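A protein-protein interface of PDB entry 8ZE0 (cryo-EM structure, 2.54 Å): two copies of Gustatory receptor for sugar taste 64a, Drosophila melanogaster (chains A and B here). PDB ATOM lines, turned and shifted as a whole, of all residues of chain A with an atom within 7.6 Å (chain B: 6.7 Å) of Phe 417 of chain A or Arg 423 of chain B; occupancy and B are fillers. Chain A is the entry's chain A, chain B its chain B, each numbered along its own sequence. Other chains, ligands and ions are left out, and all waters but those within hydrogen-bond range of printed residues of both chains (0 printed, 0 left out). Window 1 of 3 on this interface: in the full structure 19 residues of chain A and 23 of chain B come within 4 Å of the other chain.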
ATOM      1  N   LEU A 324      -2.326 -21.912  22.547  1.00  0.00           N
ATOM      2  CA  LEU A 324      -2.188 -22.006  21.097  1.00  0.00           C
ATOM      3  C   LEU A 324      -0.735 -21.840  20.673  1.00  0.00           C
ATOM      4  O   LEU A 324      -0.222 -22.614  19.856  1.00  0.00           O
ATOM      5  CB  LEU A 324      -3.061 -20.953  20.417  1.00  0.00           C
ATOM      6  CG  LEU A 324      -4.518 -21.307  20.125  1.00  0.00           C
ATOM      7  CD1 LEU A 324      -5.197 -20.141  19.431  1.00  0.00           C
ATOM      8  CD2 LEU A 324      -4.598 -22.561  19.274  1.00  0.00           C
ATOM      9  N   SER A 413      -8.407 -25.574  26.353  1.00  0.00           N
ATOM     10  CA  SER A 413      -8.617 -25.527  24.915  1.00  0.00           C
ATOM     11  C   SER A 413      -7.720 -24.471  24.287  1.00  0.00           C
ATOM     12  O   SER A 413      -7.365 -23.473  24.920  1.00  0.00           O
ATOM     13  CB  SER A 413     -10.083 -25.234  24.568  1.00  0.00           C
ATOM     14  OG  SER A 413     -10.454 -23.931  24.982  1.00  0.00           O
ATOM     15  N   GLY A 414      -7.351 -24.708  23.031  1.00  0.00           N
ATOM     16  CA  GLY A 414      -6.615 -23.735  22.251  1.00  0.00           C
ATOM     17  C   GLY A 414      -7.542 -22.785  21.522  1.00  0.00           C
ATOM     18  O   GLY A 414      -7.722 -22.900  20.306  1.00  0.00           O
ATOM     19  N   LYS A 415      -8.142 -21.850  22.263  1.00  0.00           N
ATOM     20  CA  LYS A 415      -9.143 -20.926  21.725  1.00  0.00           C
ATOM     21  C   LYS A 415     -10.330 -21.683  21.133  1.00  0.00           C
ATOM     22  O   LYS A 415     -10.861 -21.319  20.082  1.00  0.00           O
ATOM     23  CB  LYS A 415      -8.534 -19.976  20.692  1.00  0.00           C
ATOM     24  CG  LYS A 415      -8.387 -18.542  21.172  1.00  0.00           C
ATOM     25  CD  LYS A 415      -9.686 -17.770  21.014  1.00  0.00           C
ATOM     26  CE  LYS A 415      -9.443 -16.270  21.050  1.00  0.00           C
ATOM     27  NZ  LYS A 415     -10.674 -15.503  20.723  1.00  0.00           N
ATOM     28  N   LYS A 416     -10.736 -22.758  21.809  1.00  0.00           N
ATOM     29  CA  LYS A 416     -11.878 -23.606  21.479  1.00  0.00           C
ATOM     30  C   LYS A 416     -11.704 -24.363  20.168  1.00  0.00           C
ATOM     31  O   LYS A 416     -12.625 -25.085  19.764  1.00  0.00           O
ATOM     32  CB  LYS A 416     -13.193 -22.815  21.421  1.00  0.00           C
ATOM     33  CG  LYS A 416     -13.787 -22.490  22.783  1.00  0.00           C
ATOM     34  CD  LYS A 416     -13.700 -23.678  23.726  1.00  0.00           C
ATOM     35  CE  LYS A 416     -14.524 -23.443  24.982  1.00  0.00           C
ATOM     36  NZ  LYS A 416     -14.185 -22.146  25.632  1.00  0.00           N
ATOM     37  N   PHE A 417     -10.563 -24.230  19.488  1.00  0.00           N
ATOM     38  CA  PHE A 417     -10.351 -24.978  18.252  1.00  0.00           C
ATOM     39  C   PHE A 417     -10.145 -26.460  18.535  1.00  0.00           C
ATOM     40  O   PHE A 417     -10.521 -27.313  17.723  1.00  0.00           O
ATOM     41  CB  PHE A 417      -9.156 -24.404  17.492  1.00  0.00           C
ATOM     42  CG  PHE A 417      -9.396 -23.030  16.936  1.00  0.00           C
ATOM     43  CD1 PHE A 417     -10.353 -22.821  15.959  1.00  0.00           C
ATOM     44  CD2 PHE A 417      -8.662 -21.948  17.390  1.00  0.00           C
ATOM     45  CE1 PHE A 417     -10.575 -21.559  15.445  1.00  0.00           C
ATOM     46  CE2 PHE A 417      -8.879 -20.682  16.882  1.00  0.00           C
ATOM     47  CZ  PHE A 417      -9.836 -20.488  15.907  1.00  0.00           C
ATOM     48  N   TYR A 418      -9.545 -26.783  19.678  1.00  0.00           N
ATOM     49  CA  TYR A 418      -9.324 -28.160  20.089  1.00  0.00           C
ATOM     50  C   TYR A 418      -9.299 -28.205  21.608  1.00  0.00           C
ATOM     51  O   TYR A 418      -9.035 -27.198  22.269  1.00  0.00           O
ATOM     52  CB  TYR A 418      -8.020 -28.720  19.509  1.00  0.00           C
ATOM     53  CG  TYR A 418      -6.811 -27.854  19.788  1.00  0.00           C
ATOM     54  CD1 TYR A 418      -6.078 -28.006  20.958  1.00  0.00           C
ATOM     55  CD2 TYR A 418      -6.408 -26.880  18.885  1.00  0.00           C
ATOM     56  CE1 TYR A 418      -4.978 -27.214  21.219  1.00  0.00           C
ATOM     57  CE2 TYR A 418      -5.308 -26.085  19.137  1.00  0.00           C
ATOM     58  CZ  TYR A 418      -4.598 -26.256  20.305  1.00  0.00           C
ATOM     59  OH  TYR A 418      -3.504 -25.464  20.558  1.00  0.00           O
ATOM     60  N   PHE A 419      -9.569 -29.383  22.158  1.00  0.00           N
ATOM     61  CA  PHE A 419      -9.580 -29.588  23.599  1.00  0.00           C
ATOM     62  C   PHE A 419      -8.436 -30.512  23.988  1.00  0.00           C
ATOM     63  O   PHE A 419      -8.278 -31.591  23.407  1.00  0.00           O
ATOM     64  CB  PHE A 419     -10.919 -30.163  24.062  1.00  0.00           C
ATOM     65  CG  PHE A 419     -12.021 -29.144  24.126  1.00  0.00           C
ATOM     66  CD1 PHE A 419     -12.219 -28.390  25.270  1.00  0.00           C
ATOM     67  CD2 PHE A 419     -12.854 -28.936  23.040  1.00  0.00           C
ATOM     68  CE1 PHE A 419     -13.228 -27.449  25.332  1.00  0.00           C
ATOM     69  CE2 PHE A 419     -13.866 -27.998  23.096  1.00  0.00           C
ATOM     70  CZ  PHE A 419     -14.053 -27.254  24.243  1.00  0.00           C
ATOM     71  N   THR A 421      -6.946 -33.202  25.461  1.00  0.00           N
ATOM     72  CA  THR A 421      -7.329 -34.474  26.056  1.00  0.00           C
ATOM     73  C   THR A 421      -6.360 -35.550  25.589  1.00  0.00           C
ATOM     74  O   THR A 421      -5.516 -35.323  24.718  1.00  0.00           O
ATOM     75  CB  THR A 421      -8.769 -34.860  25.694  1.00  0.00           C
ATOM     76  OG1 THR A 421      -8.957 -34.740  24.278  1.00  0.00           O
ATOM     77  CG2 THR A 421      -9.762 -33.955  26.409  1.00  0.00           C
ATOM     78  N   ARG A 423      -7.288 -38.200  23.969  1.00  0.00           N
ATOM     79  CA  ARG A 423      -7.693 -38.398  22.581  1.00  0.00           C
ATOM     80  C   ARG A 423      -6.974 -37.415  21.668  1.00  0.00           C
ATOM     81  O   ARG A 423      -6.487 -37.783  20.591  1.00  0.00           O
ATOM     82  CB  ARG A 423      -9.209 -38.237  22.461  1.00  0.00           C
ATOM     83  CG  ARG A 423      -9.877 -39.158  21.455  1.00  0.00           C
ATOM     84  CD  ARG A 423      -9.616 -40.620  21.772  1.00  0.00           C
ATOM     85  NE  ARG A 423      -9.990 -41.486  20.660  1.00  0.00           N
ATOM     86  CZ  ARG A 423      -9.228 -41.719  19.601  1.00  0.00           C
ATOM     87  NH1 ARG A 423      -8.036 -41.160  19.471  1.00  0.00           N
ATOM     88  NH2 ARG A 423      -9.674 -42.531  18.648  1.00  0.00           N
ATOM     89  N   LEU A 424      -6.890 -36.151  22.091  1.00  0.00           N
ATOM     90  CA  LEU A 424      -6.175 -35.154  21.306  1.00  0.00           C
ATOM     91  C   LEU A 424      -4.687 -35.464  21.225  1.00  0.00           C
ATOM     92  O   LEU A 424      -4.069 -35.231  20.185  1.00  0.00           O
ATOM     93  CB  LEU A 424      -6.392 -33.757  21.885  1.00  0.00           C
ATOM     94  CG  LEU A 424      -5.741 -32.626  21.082  1.00  0.00           C
ATOM     95  CD1 LEU A 424      -6.666 -32.152  19.971  1.00  0.00           C
ATOM     96  CD2 LEU A 424      -5.338 -31.470  21.980  1.00  0.00           C
ATOM     97  N   LEU B 370     -15.146 -18.595  11.046  1.00  0.00           N
ATOM     98  CA  LEU B 370     -15.297 -18.167  12.433  1.00  0.00           C
ATOM     99  C   LEU B 370     -16.641 -17.487  12.665  1.00  0.00           C
ATOM    100  O   LEU B 370     -17.264 -17.681  13.712  1.00  0.00           O
ATOM    101  CB  LEU B 370     -14.149 -17.237  12.824  1.00  0.00           C
ATOM    102  CG  LEU B 370     -12.806 -17.911  13.120  1.00  0.00           C
ATOM    103  CD1 LEU B 370     -11.673 -16.897  13.088  1.00  0.00           C
ATOM    104  CD2 LEU B 370     -12.852 -18.628  14.459  1.00  0.00           C
ATOM    105  N   ALA B 373     -19.126 -20.268  12.793  1.00  0.00           N
ATOM    106  CA  ALA B 373     -18.986 -20.984  14.055  1.00  0.00           C
ATOM    107  C   ALA B 373     -19.389 -20.134  15.249  1.00  0.00           C
ATOM    108  O   ALA B 373     -19.556 -20.672  16.349  1.00  0.00           O
ATOM    109  CB  ALA B 373     -17.546 -21.464  14.228  1.00  0.00           C
ATOM    110  N   GLU B 377     -20.881 -21.341  18.848  1.00  0.00           N
ATOM    111  CA  GLU B 377     -20.298 -20.896  20.110  1.00  0.00           C
ATOM    112  C   GLU B 377     -21.312 -20.123  20.944  1.00  0.00           C
ATOM    113  O   GLU B 377     -21.359 -20.274  22.169  1.00  0.00           O
ATOM    114  CB  GLU B 377     -19.055 -20.049  19.845  1.00  0.00           C
ATOM    115  CG  GLU B 377     -17.939 -20.799  19.138  1.00  0.00           C
ATOM    116  CD  GLU B 377     -17.317 -21.874  20.008  1.00  0.00           C
ATOM    117  OE1 GLU B 377     -17.265 -21.687  21.241  1.00  0.00           O
ATOM    118  OE2 GLU B 377     -16.886 -22.910  19.460  1.00  0.00           O
ATOM    119  N   PHE B 419     -20.617 -29.440   9.429  1.00  0.00           N
ATOM    120  CA  PHE B 419     -21.170 -28.344  10.214  1.00  0.00           C
ATOM    121  C   PHE B 419     -20.087 -27.307  10.470  1.00  0.00           C
ATOM    122  O   PHE B 419     -18.991 -27.646  10.927  1.00  0.00           O
ATOM    123  CB  PHE B 419     -21.752 -28.853  11.534  1.00  0.00           C
ATOM    124  CG  PHE B 419     -23.090 -29.516  11.384  1.00  0.00           C
ATOM    125  CD1 PHE B 419     -24.256 -28.772  11.431  1.00  0.00           C
ATOM    126  CD2 PHE B 419     -23.182 -30.884  11.191  1.00  0.00           C
ATOM    127  CE1 PHE B 419     -25.489 -29.378  11.291  1.00  0.00           C
ATOM    128  CE2 PHE B 419     -24.412 -31.497  11.052  1.00  0.00           C
ATOM    129  CZ  PHE B 419     -25.567 -30.743  11.101  1.00  0.00           C
ATOM    130  N   LEU B 420     -20.398 -26.048  10.174  1.00  0.00           N
ATOM    131  CA  LEU B 420     -19.432 -24.959  10.284  1.00  0.00           C
ATOM    132  C   LEU B 420     -19.196 -24.646  11.756  1.00  0.00           C
ATOM    133  O   LEU B 420     -19.961 -23.908  12.381  1.00  0.00           O
ATOM    134  CB  LEU B 420     -19.934 -23.732   9.529  1.00  0.00           C
ATOM    135  CG  LEU B 420     -20.016 -23.886   8.007  1.00  0.00           C
ATOM    136  CD1 LEU B 420     -20.819 -22.756   7.385  1.00  0.00           C
ATOM    137  CD2 LEU B 420     -18.625 -23.946   7.401  1.00  0.00           C
ATOM    138  N   THR B 421     -18.128 -25.214  12.314  1.00  0.00           N
ATOM    139  CA  THR B 421     -17.765 -25.002  13.707  1.00  0.00           C
ATOM    140  C   THR B 421     -16.270 -24.732  13.793  1.00  0.00           C
ATOM    141  O   THR B 421     -15.536 -24.854  12.808  1.00  0.00           O
ATOM    142  CB  THR B 421     -18.139 -26.207  14.581  1.00  0.00           C
ATOM    143  OG1 THR B 421     -17.652 -27.410  13.975  1.00  0.00           O
ATOM    144  CG2 THR B 421     -19.649 -26.302  14.743  1.00  0.00           C
ATOM    145  N   ARG B 422     -15.819 -24.349  14.990  1.00  0.00           N
ATOM    146  CA  ARG B 422     -14.391 -24.146  15.213  1.00  0.00           C
ATOM    147  C   ARG B 422     -13.626 -25.455  15.066  1.00  0.00           C
ATOM    148  O   ARG B 422     -12.500 -25.472  14.552  1.00  0.00           O
ATOM    149  CB  ARG B 422     -14.160 -23.534  16.593  1.00  0.00           C
ATOM    150  CG  ARG B 422     -14.446 -22.042  16.662  1.00  0.00           C
ATOM    151  CD  ARG B 422     -14.294 -21.514  18.079  1.00  0.00           C
ATOM    152  NE  ARG B 422     -14.329 -20.057  18.129  1.00  0.00           N
ATOM    153  CZ  ARG B 422     -13.254 -19.281  18.126  1.00  0.00           C
ATOM    154  NH1 ARG B 422     -12.034 -19.790  18.082  1.00  0.00           N
ATOM    155  NH2 ARG B 422     -13.407 -17.961  18.172  1.00  0.00           N
ATOM    156  N   ARG B 423     -14.224 -26.560  15.518  1.00  0.00           N
ATOM    157  CA  ARG B 423     -13.658 -27.881  15.270  1.00  0.00           C
ATOM    158  C   ARG B 423     -13.485 -28.120  13.775  1.00  0.00           C
ATOM    159  O   ARG B 423     -12.451 -28.627  13.325  1.00  0.00           O
ATOM    160  CB  ARG B 423     -14.560 -28.951  15.886  1.00  0.00           C
ATOM    161  CG  ARG B 423     -13.832 -30.148  16.473  1.00  0.00           C
ATOM    162  CD  ARG B 423     -12.845 -29.735  17.549  1.00  0.00           C
ATOM    163  NE  ARG B 423     -11.940 -30.823  17.898  1.00  0.00           N
ATOM    164  CZ  ARG B 423     -10.851 -31.141  17.212  1.00  0.00           C
ATOM    165  NH1 ARG B 423     -10.499 -30.473  16.125  1.00  0.00           N
ATOM    166  NH2 ARG B 423     -10.097 -32.155  17.625  1.00  0.00           N
ATOM    167  N   LEU B 424     -14.497 -27.744  12.987  1.00  0.00           N
ATOM    168  CA  LEU B 424     -14.398 -27.887  11.540  1.00  0.00           C
ATOM    169  C   LEU B 424     -13.315 -26.988  10.961  1.00  0.00           C
ATOM    170  O   LEU B 424     -12.631 -27.386  10.016  1.00  0.00           O
ATOM    171  CB  LEU B 424     -15.742 -27.588  10.878  1.00  0.00           C
ATOM    172  CG  LEU B 424     -15.761 -27.785   9.359  1.00  0.00           C
ATOM    173  CD1 LEU B 424     -16.073 -29.232   9.007  1.00  0.00           C
ATOM    174  CD2 LEU B 424     -16.745 -26.841   8.690  1.00  0.00           C
ATOM    175  N   LEU B 425     -13.145 -25.780  11.502  1.00  0.00           N
ATOM    176  CA  LEU B 425     -12.080 -24.906  11.017  1.00  0.00           C
ATOM    177  C   LEU B 425     -10.705 -25.502  11.294  1.00  0.00           C
ATOM    178  O   LEU B 425      -9.818 -25.459  10.431  1.00  0.00           O
ATOM    179  CB  LEU B 425     -12.203 -23.521  11.653  1.00  0.00           C
ATOM    180  CG  LEU B 425     -11.166 -22.488  11.209  1.00  0.00           C
ATOM    181  CD1 LEU B 425     -11.131 -22.376   9.693  1.00  0.00           C
ATOM    182  CD2 LEU B 425     -11.449 -21.137  11.844  1.00  0.00           C
ATOM    183  N   PHE B 426     -10.506 -26.062  12.490  1.00  0.00           N
ATOM    184  CA  PHE B 426      -9.231 -26.706  12.798  1.00  0.00           C
ATOM    185  C   PHE B 426      -8.995 -27.920  11.906  1.00  0.00           C
ATOM    186  O   PHE B 426      -7.877 -28.140  11.418  1.00  0.00           O
ATOM    187  CB  PHE B 426      -9.187 -27.102  14.273  1.00  0.00           C
ATOM    188  CG  PHE B 426      -7.865 -27.665  14.710  1.00  0.00           C
ATOM    189  CD1 PHE B 426      -6.692 -26.970  14.476  1.00  0.00           C
ATOM    190  CD2 PHE B 426      -7.798 -28.887  15.356  1.00  0.00           C
ATOM    191  CE1 PHE B 426      -5.474 -27.484  14.877  1.00  0.00           C
ATOM    192  CE2 PHE B 426      -6.584 -29.406  15.760  1.00  0.00           C
ATOM    193  CZ  PHE B 426      -5.420 -28.703  15.520  1.00  0.00           C
ATOM    194  N   GLY B 427     -10.039 -28.721  11.682  1.00  0.00           N
ATOM    195  CA  GLY B 427      -9.906 -29.856  10.783  1.00  0.00           C
ATOM    196  C   GLY B 427      -9.588 -29.437   9.360  1.00  0.00           C
ATOM    197  O   GLY B 427      -8.795 -30.084   8.674  1.00  0.00           O
ATOM    198  N   MET B 428     -10.200 -28.344   8.900  1.00  0.00           N
ATOM    199  CA  MET B 428      -9.908 -27.831   7.566  1.00  0.00           C
ATOM    200  C   MET B 428      -8.477 -27.323   7.475  1.00  0.00           C
ATOM    201  O   MET B 428      -7.813 -27.511   6.450  1.00  0.00           O
ATOM    202  CB  MET B 428     -10.897 -26.724   7.201  1.00  0.00           C
ATOM    203  CG  MET B 428     -10.423 -25.814   6.080  1.00  0.00           C
ATOM    204  SD  MET B 428     -11.402 -24.313   5.912  1.00  0.00           S
ATOM    205  CE  MET B 428     -11.227 -23.996   4.159  1.00  0.00           C
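The backbone carbonyl oxygen of Lys 415 of chain A lies within hydrogen-bond range of the guanidinium group of Arg 422 of chain B (2.8 Å).
The side-chain hydroxyl of Ser 413 of chain A sits at hydrogen-bond distance from the backbone NH of Lys 416 of chain A.
Among the printed residues, merely in contact across the chains: Phe 417 of chain A with Arg 422 of chain B (3.2 Å), Phe 417 of chain A with Arg 423 of chain B (3.4 Å), Phe 417 of chain A with Phe 426 of chain B (3.7 Å), Phe 417 of chain A with Leu 425 of chain B (3.7 Å), Lys 416 of chain A with Arg 422 of chain B (3.8 Å), Phe 417 of chain A with Leu 370 of chain B (3.8 Å), Lys 416 of chain A with Glu 377 of chain B (3.9 Å) and Tyr 418 of chain A with Phe 426 of chain B (3.95 Å).
Of the printed residues of chain B, Phe 417 of chain A touches Leu 370, Arg 422, Arg 423, Leu 425 and Phe 426. Of the printed residues of chain A, Arg 422 of chain B touches Lys 415 (2.8 Å), Lys 416 (3.8 Å) and Phe 417 (3.2 Å). Printed residues of chain B within 4 Å of Lys 416 of chain A: Glu 377 and Arg 422. Leu 424 of chain A touches none of the printed residues of chain B.
Hydrophobic or aromatic side chains of chain B that line the printed part of chain A: Leu 370, Leu 425 and Phe 426. Hydrophobic or aromatic side chains of chain A within 4 Å of the printed part of chain B: Phe 417 and Tyr 418. Among the printed residues, no Asp or Glu carboxylate lies within 4 Å of a Lys or Arg side-chain nitrogen of the other chain.
4 positions are printed for both chains. Of the 9 pairs that touch across the chains among the printed residues, none has its exchanged pair printed and touching as well.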
